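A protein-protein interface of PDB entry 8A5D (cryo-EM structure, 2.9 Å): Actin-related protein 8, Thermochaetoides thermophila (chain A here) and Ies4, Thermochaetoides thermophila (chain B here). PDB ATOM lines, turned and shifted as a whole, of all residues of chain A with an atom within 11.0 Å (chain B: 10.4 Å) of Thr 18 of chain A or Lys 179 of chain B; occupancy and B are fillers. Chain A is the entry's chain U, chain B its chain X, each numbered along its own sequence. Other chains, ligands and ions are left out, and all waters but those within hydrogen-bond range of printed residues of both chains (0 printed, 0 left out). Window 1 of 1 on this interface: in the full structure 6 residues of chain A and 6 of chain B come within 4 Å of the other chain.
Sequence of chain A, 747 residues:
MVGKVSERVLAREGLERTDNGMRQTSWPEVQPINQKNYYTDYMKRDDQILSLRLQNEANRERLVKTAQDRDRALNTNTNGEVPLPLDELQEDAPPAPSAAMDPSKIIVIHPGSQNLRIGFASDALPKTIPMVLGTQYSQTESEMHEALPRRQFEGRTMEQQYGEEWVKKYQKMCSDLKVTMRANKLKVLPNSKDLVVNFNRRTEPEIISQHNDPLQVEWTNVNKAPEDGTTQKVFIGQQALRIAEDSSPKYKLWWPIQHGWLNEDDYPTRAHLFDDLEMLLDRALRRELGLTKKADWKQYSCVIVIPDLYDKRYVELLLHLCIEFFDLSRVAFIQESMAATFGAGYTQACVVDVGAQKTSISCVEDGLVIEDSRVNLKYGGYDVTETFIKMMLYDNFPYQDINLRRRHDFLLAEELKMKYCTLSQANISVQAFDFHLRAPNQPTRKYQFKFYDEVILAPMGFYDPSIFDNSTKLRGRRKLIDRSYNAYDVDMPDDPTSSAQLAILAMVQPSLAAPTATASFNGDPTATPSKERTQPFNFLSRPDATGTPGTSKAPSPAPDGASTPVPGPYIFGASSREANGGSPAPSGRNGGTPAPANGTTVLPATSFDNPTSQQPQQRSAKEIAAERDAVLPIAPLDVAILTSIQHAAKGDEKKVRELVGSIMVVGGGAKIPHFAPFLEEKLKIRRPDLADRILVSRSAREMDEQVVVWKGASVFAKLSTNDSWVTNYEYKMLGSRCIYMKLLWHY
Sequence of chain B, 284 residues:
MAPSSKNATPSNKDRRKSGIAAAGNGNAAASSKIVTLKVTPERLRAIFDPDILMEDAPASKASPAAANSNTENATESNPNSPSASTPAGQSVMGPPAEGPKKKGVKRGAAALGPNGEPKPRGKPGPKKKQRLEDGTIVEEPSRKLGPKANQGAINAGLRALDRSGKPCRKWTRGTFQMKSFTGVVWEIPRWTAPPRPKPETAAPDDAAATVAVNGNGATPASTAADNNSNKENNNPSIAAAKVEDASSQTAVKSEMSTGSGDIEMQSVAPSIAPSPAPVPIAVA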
ATOM      1  N   GLU A   7     -29.146 -23.581 -21.064  1.00  0.00           N
ATOM      2  CA  GLU A   7     -28.109 -24.449 -20.424  1.00  0.00           C
ATOM      3  C   GLU A   7     -26.743 -24.342 -21.127  1.00  0.00           C
ATOM      4  O   GLU A   7     -25.734 -24.165 -20.412  1.00  0.00           O
ATOM      5  CB  GLU A   7     -28.595 -25.902 -20.370  1.00  0.00           C
ATOM      6  CG  GLU A   7     -27.675 -26.847 -19.604  1.00  0.00           C
ATOM      7  CD  GLU A   7     -27.444 -26.540 -18.129  1.00  0.00           C
ATOM      8  OE1 GLU A   7     -26.426 -27.017 -17.584  1.00  0.00           O
ATOM      9  OE2 GLU A   7     -28.280 -25.838 -17.521  1.00  0.00           O
ATOM     10  N   ALA A  11     -22.912 -23.454 -19.733  1.00  0.00           N
ATOM     11  CA  ALA A  11     -21.786 -24.391 -19.973  1.00  0.00           C
ATOM     12  C   ALA A  11     -20.664 -23.690 -20.763  1.00  0.00           C
ATOM     13  O   ALA A  11     -19.484 -23.939 -20.432  1.00  0.00           O
ATOM     14  CB  ALA A  11     -22.281 -25.637 -20.672  1.00  0.00           C
ATOM     15  N   GLY A  14     -18.775 -21.707 -18.587  1.00  0.00           N
ATOM     16  CA  GLY A  14     -18.062 -22.654 -17.707  1.00  0.00           C
ATOM     17  C   GLY A  14     -18.785 -22.876 -16.391  1.00  0.00           C
ATOM     18  O   GLY A  14     -18.161 -23.486 -15.495  1.00  0.00           O
ATOM     19  N   LEU A  15     -20.051 -22.456 -16.273  1.00  0.00           N
ATOM     20  CA  LEU A  15     -20.831 -22.549 -15.007  1.00  0.00           C
ATOM     21  C   LEU A  15     -21.763 -23.773 -15.053  1.00  0.00           C
ATOM     22  O   LEU A  15     -22.555 -23.904 -15.994  1.00  0.00           O
ATOM     23  CB  LEU A  15     -21.619 -21.261 -14.765  1.00  0.00           C
ATOM     24  CG  LEU A  15     -20.861 -19.944 -14.923  1.00  0.00           C
ATOM     25  CD1 LEU A  15     -21.803 -18.761 -14.754  1.00  0.00           C
ATOM     26  CD2 LEU A  15     -19.706 -19.828 -13.949  1.00  0.00           C
ATOM     27  N   GLU A  16     -21.667 -24.647 -14.053  1.00  0.00           N
ATOM     28  CA  GLU A  16     -22.372 -25.953 -14.033  1.00  0.00           C
ATOM     29  C   GLU A  16     -22.488 -26.474 -12.596  1.00  0.00           C
ATOM     30  O   GLU A  16     -21.464 -26.618 -11.917  1.00  0.00           O
ATOM     31  CB  GLU A  16     -21.625 -26.936 -14.929  1.00  0.00           C
ATOM     32  CG  GLU A  16     -22.105 -28.378 -14.794  1.00  0.00           C
ATOM     33  CD  GLU A  16     -21.670 -29.291 -15.930  1.00  0.00           C
ATOM     34  OE1 GLU A  16     -20.538 -29.114 -16.437  1.00  0.00           O
ATOM     35  OE2 GLU A  16     -22.470 -30.173 -16.311  1.00  0.00           O
ATOM     36  N   ARG A  17     -23.705 -26.780 -12.154  1.00  0.00           N
ATOM     37  CA  ARG A  17     -23.944 -27.304 -10.786  1.00  0.00           C
ATOM     38  C   ARG A  17     -23.700 -28.817 -10.784  1.00  0.00           C
ATOM     39  O   ARG A  17     -23.985 -29.491 -11.798  1.00  0.00           O
ATOM     40  CB  ARG A  17     -25.301 -26.859 -10.232  1.00  0.00           C
ATOM     41  CG  ARG A  17     -26.538 -27.493 -10.849  1.00  0.00           C
ATOM     42  CD  ARG A  17     -27.764 -27.011 -10.091  1.00  0.00           C
ATOM     43  NE  ARG A  17     -28.934 -27.877 -10.250  1.00  0.00           N
ATOM     44  CZ  ARG A  17     -29.874 -28.113  -9.323  1.00  0.00           C
ATOM     45  NH1 ARG A  17     -29.808 -27.559  -8.119  1.00  0.00           N
ATOM     46  NH2 ARG A  17     -30.880 -28.925  -9.607  1.00  0.00           N
ATOM     47  N   THR A  18     -23.164 -29.311  -9.665  1.00  0.00           N
ATOM     48  CA  THR A  18     -22.410 -30.588  -9.571  1.00  0.00           C
ATOM     49  C   THR A  18     -22.587 -31.239  -8.194  1.00  0.00           C
ATOM     50  O   THR A  18     -22.670 -30.543  -7.153  1.00  0.00           O
ATOM     51  CB  THR A  18     -20.933 -30.364  -9.929  1.00  0.00           C
ATOM     52  OG1 THR A  18     -20.305 -31.647  -9.888  1.00  0.00           O
ATOM     53  CG2 THR A  18     -20.203 -29.387  -9.026  1.00  0.00           C
ATOM     54  N   ASP A  19     -22.594 -32.566  -8.199  1.00  0.00           N
ATOM     55  CA  ASP A  19     -22.736 -33.412  -6.989  1.00  0.00           C
ATOM     56  C   ASP A  19     -21.366 -33.552  -6.302  1.00  0.00           C
ATOM     57  O   ASP A  19     -21.327 -33.970  -5.118  1.00  0.00           O
ATOM     58  CB  ASP A  19     -23.259 -34.813  -7.356  1.00  0.00           C
ATOM     59  CG  ASP A  19     -24.491 -34.894  -8.253  1.00  0.00           C
ATOM     60  OD1 ASP A  19     -25.383 -34.028  -8.119  1.00  0.00           O
ATOM     61  OD2 ASP A  19     -24.565 -35.855  -9.066  1.00  0.00           O
ATOM     62  N   ASN A  20     -20.269 -33.371  -7.047  1.00  0.00           N
ATOM     63  CA  ASN A  20     -18.886 -33.769  -6.665  1.00  0.00           C
ATOM     64  C   ASN A  20     -18.826 -35.253  -6.232  1.00  0.00           C
ATOM     65  O   ASN A  20     -17.881 -35.630  -5.513  1.00  0.00           O
ATOM     66  CB  ASN A  20     -18.344 -32.789  -5.633  1.00  0.00           C
ATOM     67  CG  ASN A  20     -17.839 -31.506  -6.244  1.00  0.00           C
ATOM     68  OD1 ASN A  20     -16.919 -31.533  -7.060  1.00  0.00           O
ATOM     69  ND2 ASN A  20     -18.409 -30.382  -5.828  1.00  0.00           N
ATOM     70  N   GLY A  21     -19.750 -36.092  -6.710  1.00  0.00           N
ATOM     71  CA  GLY A  21     -19.817 -37.535  -6.407  1.00  0.00           C
ATOM     72  C   GLY A  21     -20.073 -37.838  -4.945  1.00  0.00           C
ATOM     73  O   GLY A  21     -20.035 -39.026  -4.574  1.00  0.00           O
ATOM     74  N   MET A  22     -20.431 -36.829  -4.159  1.00  0.00           N
ATOM     75  CA  MET A  22     -20.705 -36.952  -2.706  1.00  0.00           C
ATOM     76  C   MET A  22     -22.096 -37.562  -2.477  1.00  0.00           C
ATOM     77  O   MET A  22     -22.999 -37.419  -3.338  1.00  0.00           O
ATOM     78  CB  MET A  22     -20.688 -35.570  -2.058  1.00  0.00           C
ATOM     79  CG  MET A  22     -19.361 -34.874  -2.183  1.00  0.00           C
ATOM     80  SD  MET A  22     -18.155 -35.721  -1.134  1.00  0.00           S
ATOM     81  CE  MET A  22     -16.753 -34.617  -1.262  1.00  0.00           C
ATOM     82  N   ARG A  23     -22.262 -38.173  -1.312  1.00  0.00           N
ATOM     83  CA  ARG A  23     -23.576 -38.539  -0.737  1.00  0.00           C
ATOM     84  C   ARG A  23     -24.309 -37.245  -0.370  1.00  0.00           C
ATOM     85  O   ARG A  23     -23.599 -36.209  -0.219  1.00  0.00           O
ATOM     86  CB  ARG A  23     -23.363 -39.463   0.467  1.00  0.00           C
ATOM     87  CG  ARG A  23     -22.770 -40.811   0.084  1.00  0.00           C
ATOM     88  CD  ARG A  23     -22.671 -41.801   1.232  1.00  0.00           C
ATOM     89  NE  ARG A  23     -21.891 -41.312   2.371  1.00  0.00           N
ATOM     90  CZ  ARG A  23     -20.556 -41.346   2.497  1.00  0.00           C
ATOM     91  NH1 ARG A  23     -19.780 -41.831   1.533  1.00  0.00           N
ATOM     92  NH2 ARG A  23     -20.008 -40.862   3.602  1.00  0.00           N
ATOM     93  N   GLN A  24     -25.648 -37.321  -0.190  1.00  0.00           N
ATOM     94  CA  GLN A  24     -26.502 -36.186   0.260  1.00  0.00           C
ATOM     95  C   GLN A  24     -25.871 -35.511   1.480  1.00  0.00           C
ATOM     96  O   GLN A  24     -25.851 -34.258   1.506  1.00  0.00           O
ATOM     97  CB  GLN A  24     -27.928 -36.598   0.623  1.00  0.00           C
ATOM     98  CG  GLN A  24     -28.764 -35.449   1.184  1.00  0.00           C
ATOM     99  CD  GLN A  24     -30.220 -35.808   1.309  1.00  0.00           C
ATOM    100  OE1 GLN A  24     -30.709 -36.792   0.748  1.00  0.00           O
ATOM    101  NE2 GLN A  24     -30.932 -34.995   2.064  1.00  0.00           N
ATOM    102  N   PHE B 176      -8.237 -36.109  -3.639  1.00  0.00           N
ATOM    103  CA  PHE B 176      -9.510 -36.185  -4.384  1.00  0.00           C
ATOM    104  C   PHE B 176      -9.722 -34.841  -5.056  1.00  0.00           C
ATOM    105  O   PHE B 176      -9.715 -33.811  -4.356  1.00  0.00           O
ATOM    106  CB  PHE B 176     -10.631 -36.514  -3.430  1.00  0.00           C
ATOM    107  CG  PHE B 176     -11.973 -36.673  -4.071  1.00  0.00           C
ATOM    108  CD1 PHE B 176     -12.178 -37.634  -5.038  1.00  0.00           C
ATOM    109  CD2 PHE B 176     -13.052 -35.936  -3.619  1.00  0.00           C
ATOM    110  CE1 PHE B 176     -13.432 -37.823  -5.583  1.00  0.00           C
ATOM    111  CE2 PHE B 176     -14.309 -36.133  -4.159  1.00  0.00           C
ATOM    112  CZ  PHE B 176     -14.494 -37.071  -5.144  1.00  0.00           C
ATOM    113  N   GLN B 177      -9.839 -34.863  -6.387  1.00  0.00           N
ATOM    114  CA  GLN B 177     -10.147 -33.671  -7.206  1.00  0.00           C
ATOM    115  C   GLN B 177     -11.632 -33.379  -7.068  1.00  0.00           C
ATOM    116  O   GLN B 177     -12.456 -34.315  -7.253  1.00  0.00           O
ATOM    117  CB  GLN B 177      -9.768 -33.904  -8.663  1.00  0.00           C
ATOM    118  CG  GLN B 177      -8.265 -33.867  -8.868  1.00  0.00           C
ATOM    119  CD  GLN B 177      -7.924 -33.775 -10.334  1.00  0.00           C
ATOM    120  OE1 GLN B 177      -7.256 -32.842 -10.775  1.00  0.00           O
ATOM    121  NE2 GLN B 177      -8.410 -34.735 -11.106  1.00  0.00           N
ATOM    122  N   MET B 178     -11.963 -32.119  -6.792  1.00  0.00           N
ATOM    123  CA  MET B 178     -13.373 -31.694  -6.743  1.00  0.00           C
ATOM    124  C   MET B 178     -13.528 -30.276  -7.294  1.00  0.00           C
ATOM    125  O   MET B 178     -12.504 -29.573  -7.487  1.00  0.00           O
ATOM    126  CB  MET B 178     -13.919 -31.828  -5.328  1.00  0.00           C
ATOM    127  CG  MET B 178     -13.273 -30.958  -4.304  1.00  0.00           C
ATOM    128  SD  MET B 178     -14.459 -30.812  -2.966  1.00  0.00           S
ATOM    129  CE  MET B 178     -14.606 -32.539  -2.532  1.00  0.00           C
ATOM    130  N   LYS B 179     -14.756 -29.924  -7.662  1.00  0.00           N
ATOM    131  CA  LYS B 179     -14.992 -28.850  -8.645  1.00  0.00           C
ATOM    132  C   LYS B 179     -16.034 -27.888  -8.092  1.00  0.00           C
ATOM    133  O   LYS B 179     -17.105 -28.340  -7.684  1.00  0.00           O
ATOM    134  CB  LYS B 179     -15.397 -29.476  -9.980  1.00  0.00           C
ATOM    135  CG  LYS B 179     -15.218 -28.580 -11.193  1.00  0.00           C
ATOM    136  CD  LYS B 179     -15.650 -29.269 -12.481  1.00  0.00           C
ATOM    137  CE  LYS B 179     -14.778 -30.449 -12.870  1.00  0.00           C
ATOM    138  NZ  LYS B 179     -15.284 -31.139 -14.083  1.00  0.00           N
ATOM    139  N   SER B 180     -15.728 -26.596  -8.160  1.00  0.00           N
ATOM    140  CA  SER B 180     -16.687 -25.497  -7.914  1.00  0.00           C
ATOM    141  C   SER B 180     -17.669 -25.332  -9.079  1.00  0.00           C
ATOM    142  O   SER B 180     -17.373 -25.725 -10.213  1.00  0.00           O
ATOM    143  CB  SER B 180     -15.935 -24.235  -7.701  1.00  0.00           C
ATOM    144  OG  SER B 180     -15.185 -23.912  -8.848  1.00  0.00           O
ATOM    145  N   PHE B 181     -18.800 -24.692  -8.834  1.00  0.00           N
ATOM    146  CA  PHE B 181     -19.836 -24.473  -9.873  1.00  0.00           C
ATOM    147  C   PHE B 181     -19.313 -23.481 -10.921  1.00  0.00           C
ATOM    148  O   PHE B 181     -19.873 -23.460 -12.005  1.00  0.00           O
ATOM    149  CB  PHE B 181     -21.162 -24.096  -9.211  1.00  0.00           C
ATOM    150  CG  PHE B 181     -21.284 -22.666  -8.794  1.00  0.00           C
ATOM    151  CD1 PHE B 181     -21.045 -22.288  -7.494  1.00  0.00           C
ATOM    152  CD2 PHE B 181     -21.700 -21.708  -9.700  1.00  0.00           C
ATOM    153  CE1 PHE B 181     -21.192 -20.966  -7.116  1.00  0.00           C
ATOM    154  CE2 PHE B 181     -21.847 -20.385  -9.322  1.00  0.00           C
ATOM    155  CZ  PHE B 181     -21.583 -20.017  -8.032  1.00  0.00           C
ATOM    156  N   THR B 182     -18.295 -22.680 -10.612  1.00  0.00           N
ATOM    157  CA  THR B 182     -17.607 -21.785 -11.582  1.00  0.00           C
ATOM    158  C   THR B 182     -16.427 -22.491 -12.297  1.00  0.00           C
ATOM    159  O   THR B 182     -15.564 -21.797 -12.932  1.00  0.00           O
ATOM    160  CB  THR B 182     -17.145 -20.506 -10.876  1.00  0.00           C
ATOM    161  OG1 THR B 182     -16.171 -20.814  -9.871  1.00  0.00           O
ATOM    162  CG2 THR B 182     -18.313 -19.772 -10.253  1.00  0.00           C
ATOM    163  N   GLY B 183     -16.333 -23.813 -12.180  1.00  0.00           N
ATOM    164  CA  GLY B 183     -15.423 -24.642 -12.985  1.00  0.00           C
ATOM    165  C   GLY B 183     -14.003 -24.748 -12.454  1.00  0.00           C
ATOM    166  O   GLY B 183     -13.220 -25.488 -13.088  1.00  0.00           O
ATOM    167  N   VAL B 184     -13.654 -24.075 -11.351  1.00  0.00           N
ATOM    168  CA  VAL B 184     -12.289 -24.183 -10.744  1.00  0.00           C
ATOM    169  C   VAL B 184     -12.172 -25.515  -9.991  1.00  0.00           C
ATOM    170  O   VAL B 184     -13.104 -25.850  -9.233  1.00  0.00           O
ATOM    171  CB  VAL B 184     -11.935 -23.005  -9.831  1.00  0.00           C
ATOM    172  CG1 VAL B 184     -10.505 -23.126  -9.352  1.00  0.00           C
ATOM    173  CG2 VAL B 184     -12.134 -21.676 -10.536  1.00  0.00           C
ATOM    174  N   VAL B 185     -11.060 -26.227 -10.227  1.00  0.00           N
ATOM    175  CA  VAL B 185     -10.759 -27.586  -9.687  1.00  0.00           C
ATOM    176  C   VAL B 185      -9.728 -27.476  -8.573  1.00  0.00           C
ATOM    177  O   VAL B 185      -8.699 -26.786  -8.767  1.00  0.00           O
ATOM    178  CB  VAL B 185     -10.264 -28.540 -10.784  1.00  0.00           C
ATOM    179  CG1 VAL B 185      -9.756 -29.850 -10.199  1.00  0.00           C
ATOM    180  CG2 VAL B 185     -11.357 -28.808 -11.810  1.00  0.00           C
ATOM    181  N   TRP B 186      -9.991 -28.151  -7.449  1.00  0.00           N
ATOM    182  CA  TRP B 186      -9.072 -28.141  -6.284  1.00  0.00           C
ATOM    183  C   TRP B 186      -9.026 -29.506  -5.603  1.00  0.00           C
ATOM    184  O   TRP B 186      -9.874 -30.357  -5.905  1.00  0.00           O
ATOM    185  CB  TRP B 186      -9.453 -27.006  -5.331  1.00  0.00           C
ATOM    186  CG  TRP B 186     -10.825 -27.079  -4.740  1.00  0.00           C
ATOM    187  CD1 TRP B 186     -11.984 -26.733  -5.351  1.00  0.00           C
ATOM    188  CD2 TRP B 186     -11.187 -27.487  -3.407  1.00  0.00           C
ATOM    189  NE1 TRP B 186     -13.048 -26.941  -4.517  1.00  0.00           N
ATOM    190  CE2 TRP B 186     -12.596 -27.405  -3.314  1.00  0.00           C
ATOM    191  CE3 TRP B 186     -10.481 -27.980  -2.304  1.00  0.00           C
ATOM    192  CZ2 TRP B 186     -13.302 -27.719  -2.150  1.00  0.00           C
ATOM    193  CZ3 TRP B 186     -11.183 -28.307  -1.160  1.00  0.00           C
ATOM    194  CH2 TRP B 186     -12.573 -28.176  -1.082  1.00  0.00           C
ATOM    195  N   GLU B 187      -8.013 -29.732  -4.761  1.00  0.00           N
ATOM    196  CA  GLU B 187      -7.735 -31.065  -4.155  1.00  0.00           C
ATOM    197  C   GLU B 187      -7.966 -31.034  -2.640  1.00  0.00           C
ATOM    198  O   GLU B 187      -7.424 -30.146  -1.939  1.00  0.00           O
ATOM    199  CB  GLU B 187      -6.320 -31.522  -4.497  1.00  0.00           C
ATOM    200  CG  GLU B 187      -6.194 -31.974  -5.946  1.00  0.00           C
ATOM    201  CD  GLU B 187      -4.774 -32.082  -6.477  1.00  0.00           C
ATOM    202  OE1 GLU B 187      -3.888 -31.351  -5.982  1.00  0.00           O
ATOM    203  OE2 GLU B 187      -4.556 -32.900  -7.391  1.00  0.00           O
ATOM    204  N   ILE B 188      -8.704 -32.026  -2.158  1.00  0.00           N
ATOM    205  CA  ILE B 188      -8.909 -32.292  -0.710  1.00  0.00           C
ATOM    206  C   ILE B 188      -8.226 -33.621  -0.373  1.00  0.00           C
ATOM    207  O   ILE B 188      -8.313 -34.595  -1.125  1.00  0.00           O
ATOM    208  CB  ILE B 188     -10.414 -32.263  -0.350  1.00  0.00           C
ATOM    209  CG1 ILE B 188     -10.598 -32.119   1.154  1.00  0.00           C
ATOM    210  CG2 ILE B 188     -11.205 -33.462  -0.876  1.00  0.00           C
ATOM    211  CD1 ILE B 188     -10.251 -30.738   1.661  1.00  0.00           C
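The backbone NH of Glu 16 of chain A sits at hydrogen-bond distance from the backbone carbonyl oxygen of Phe 181 of chain B, 3.0 Å away.
The backbone NH of Lys 179 of chain B lies within hydrogen-bond range of the side-chain amide oxygen of Asn 20 of chain A, at 2.8 Å.
Of the 13 printed residues of chain B, 6 touch a printed residue of chain A.
Printed residues of chain B that touch a printed residue of chain A: Phe 176, Met 178, Lys 179, Phe 181, Thr 182 and Gly 183.
Hydrophobic or aromatic side chains of chain B that line the printed part of chain A: Phe 176, Met 178 and Phe 181.
Hydrophobic or aromatic side chains of chain A within 4 Å of the printed part of chain B: Leu 15 and Met 22.
Among the printed residues, 11 pairs touch across the chains.
The backbone NH of Asn 20 of chain A sits at hydrogen-bond distance from the side-chain hydroxyl of Thr 18 of chain A.
N of Phe 176 of chain B sits at hydrogen-bond distance from O of Ile 188 of chain B (2.9 Å).
The backbone NH (N) of Met 178 of chain B is in hydrogen-bond range of the backbone carbonyl oxygen (O) of Trp 186 of chain B (2.9 Å).
OG of Ser 180 of chain B lies within hydrogen-bond range of OG1 of Thr 182 of chain B (3.4 Å).
Printed residues of chain B within 4 Å of Thr 18 of chain A: Lys 179.
Of chain A, only Thr 18 (3.5 Å) and Asn 20 (2.8 Å) come within 4 Å of Lys 179 of chain B.
No residue of chain B comes within 4 Å of Asp 19 of chain A.
Met 178 of chain B touches two residues of chain A.
Of the printed residues of chain A, Gly 183 of chain B touches Gly 14.
No residue of chain A comes within 4 Å of Val 185 of chain B.
Of the printed residues of chain B, Met 22 of chain A touches Met 178.
Printed residues of chain A within 4 Å of Phe 176 of chain B: Asn 20 (3.7 Å).
Printed residues of chain B within 4 Å of Glu 16 of chain A: Phe 181 (3.0 Å).
Gln 177 of chain B touches none of the printed residues of chain A.
The nearest residue of chain B that does not touch Thr 18 of chain A is Ser 180 of chain B (4.8 Å).
The nearest residue of chain A that does not touch Lys 179 of chain B is Glu 16 of chain A (6.1 Å).
Among the printed residues, pairs that only touch across the chains: Gly 14 of chain A with Phe 181 of chain B (3.9 Å), Gly 14 of chain A with Thr 182 of chain B (3.8 Å), Gly 14 of chain A with Gly 183 of chain B (3.8 Å), Leu 15 of chain A with Phe 181 of chain B (3.3 Å), Leu 15 of chain A with Thr 182 of chain B (3.7 Å), Thr 18 of chain A with Lys 179 of chain B (3.5 Å), Asn 20 of chain A with Phe 176 of chain B (3.7 Å), Asn 20 of chain A with Met 178 of chain B (3.5 Å) and Met 22 of chain A with Met 178 of chain B (3.2 Å).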
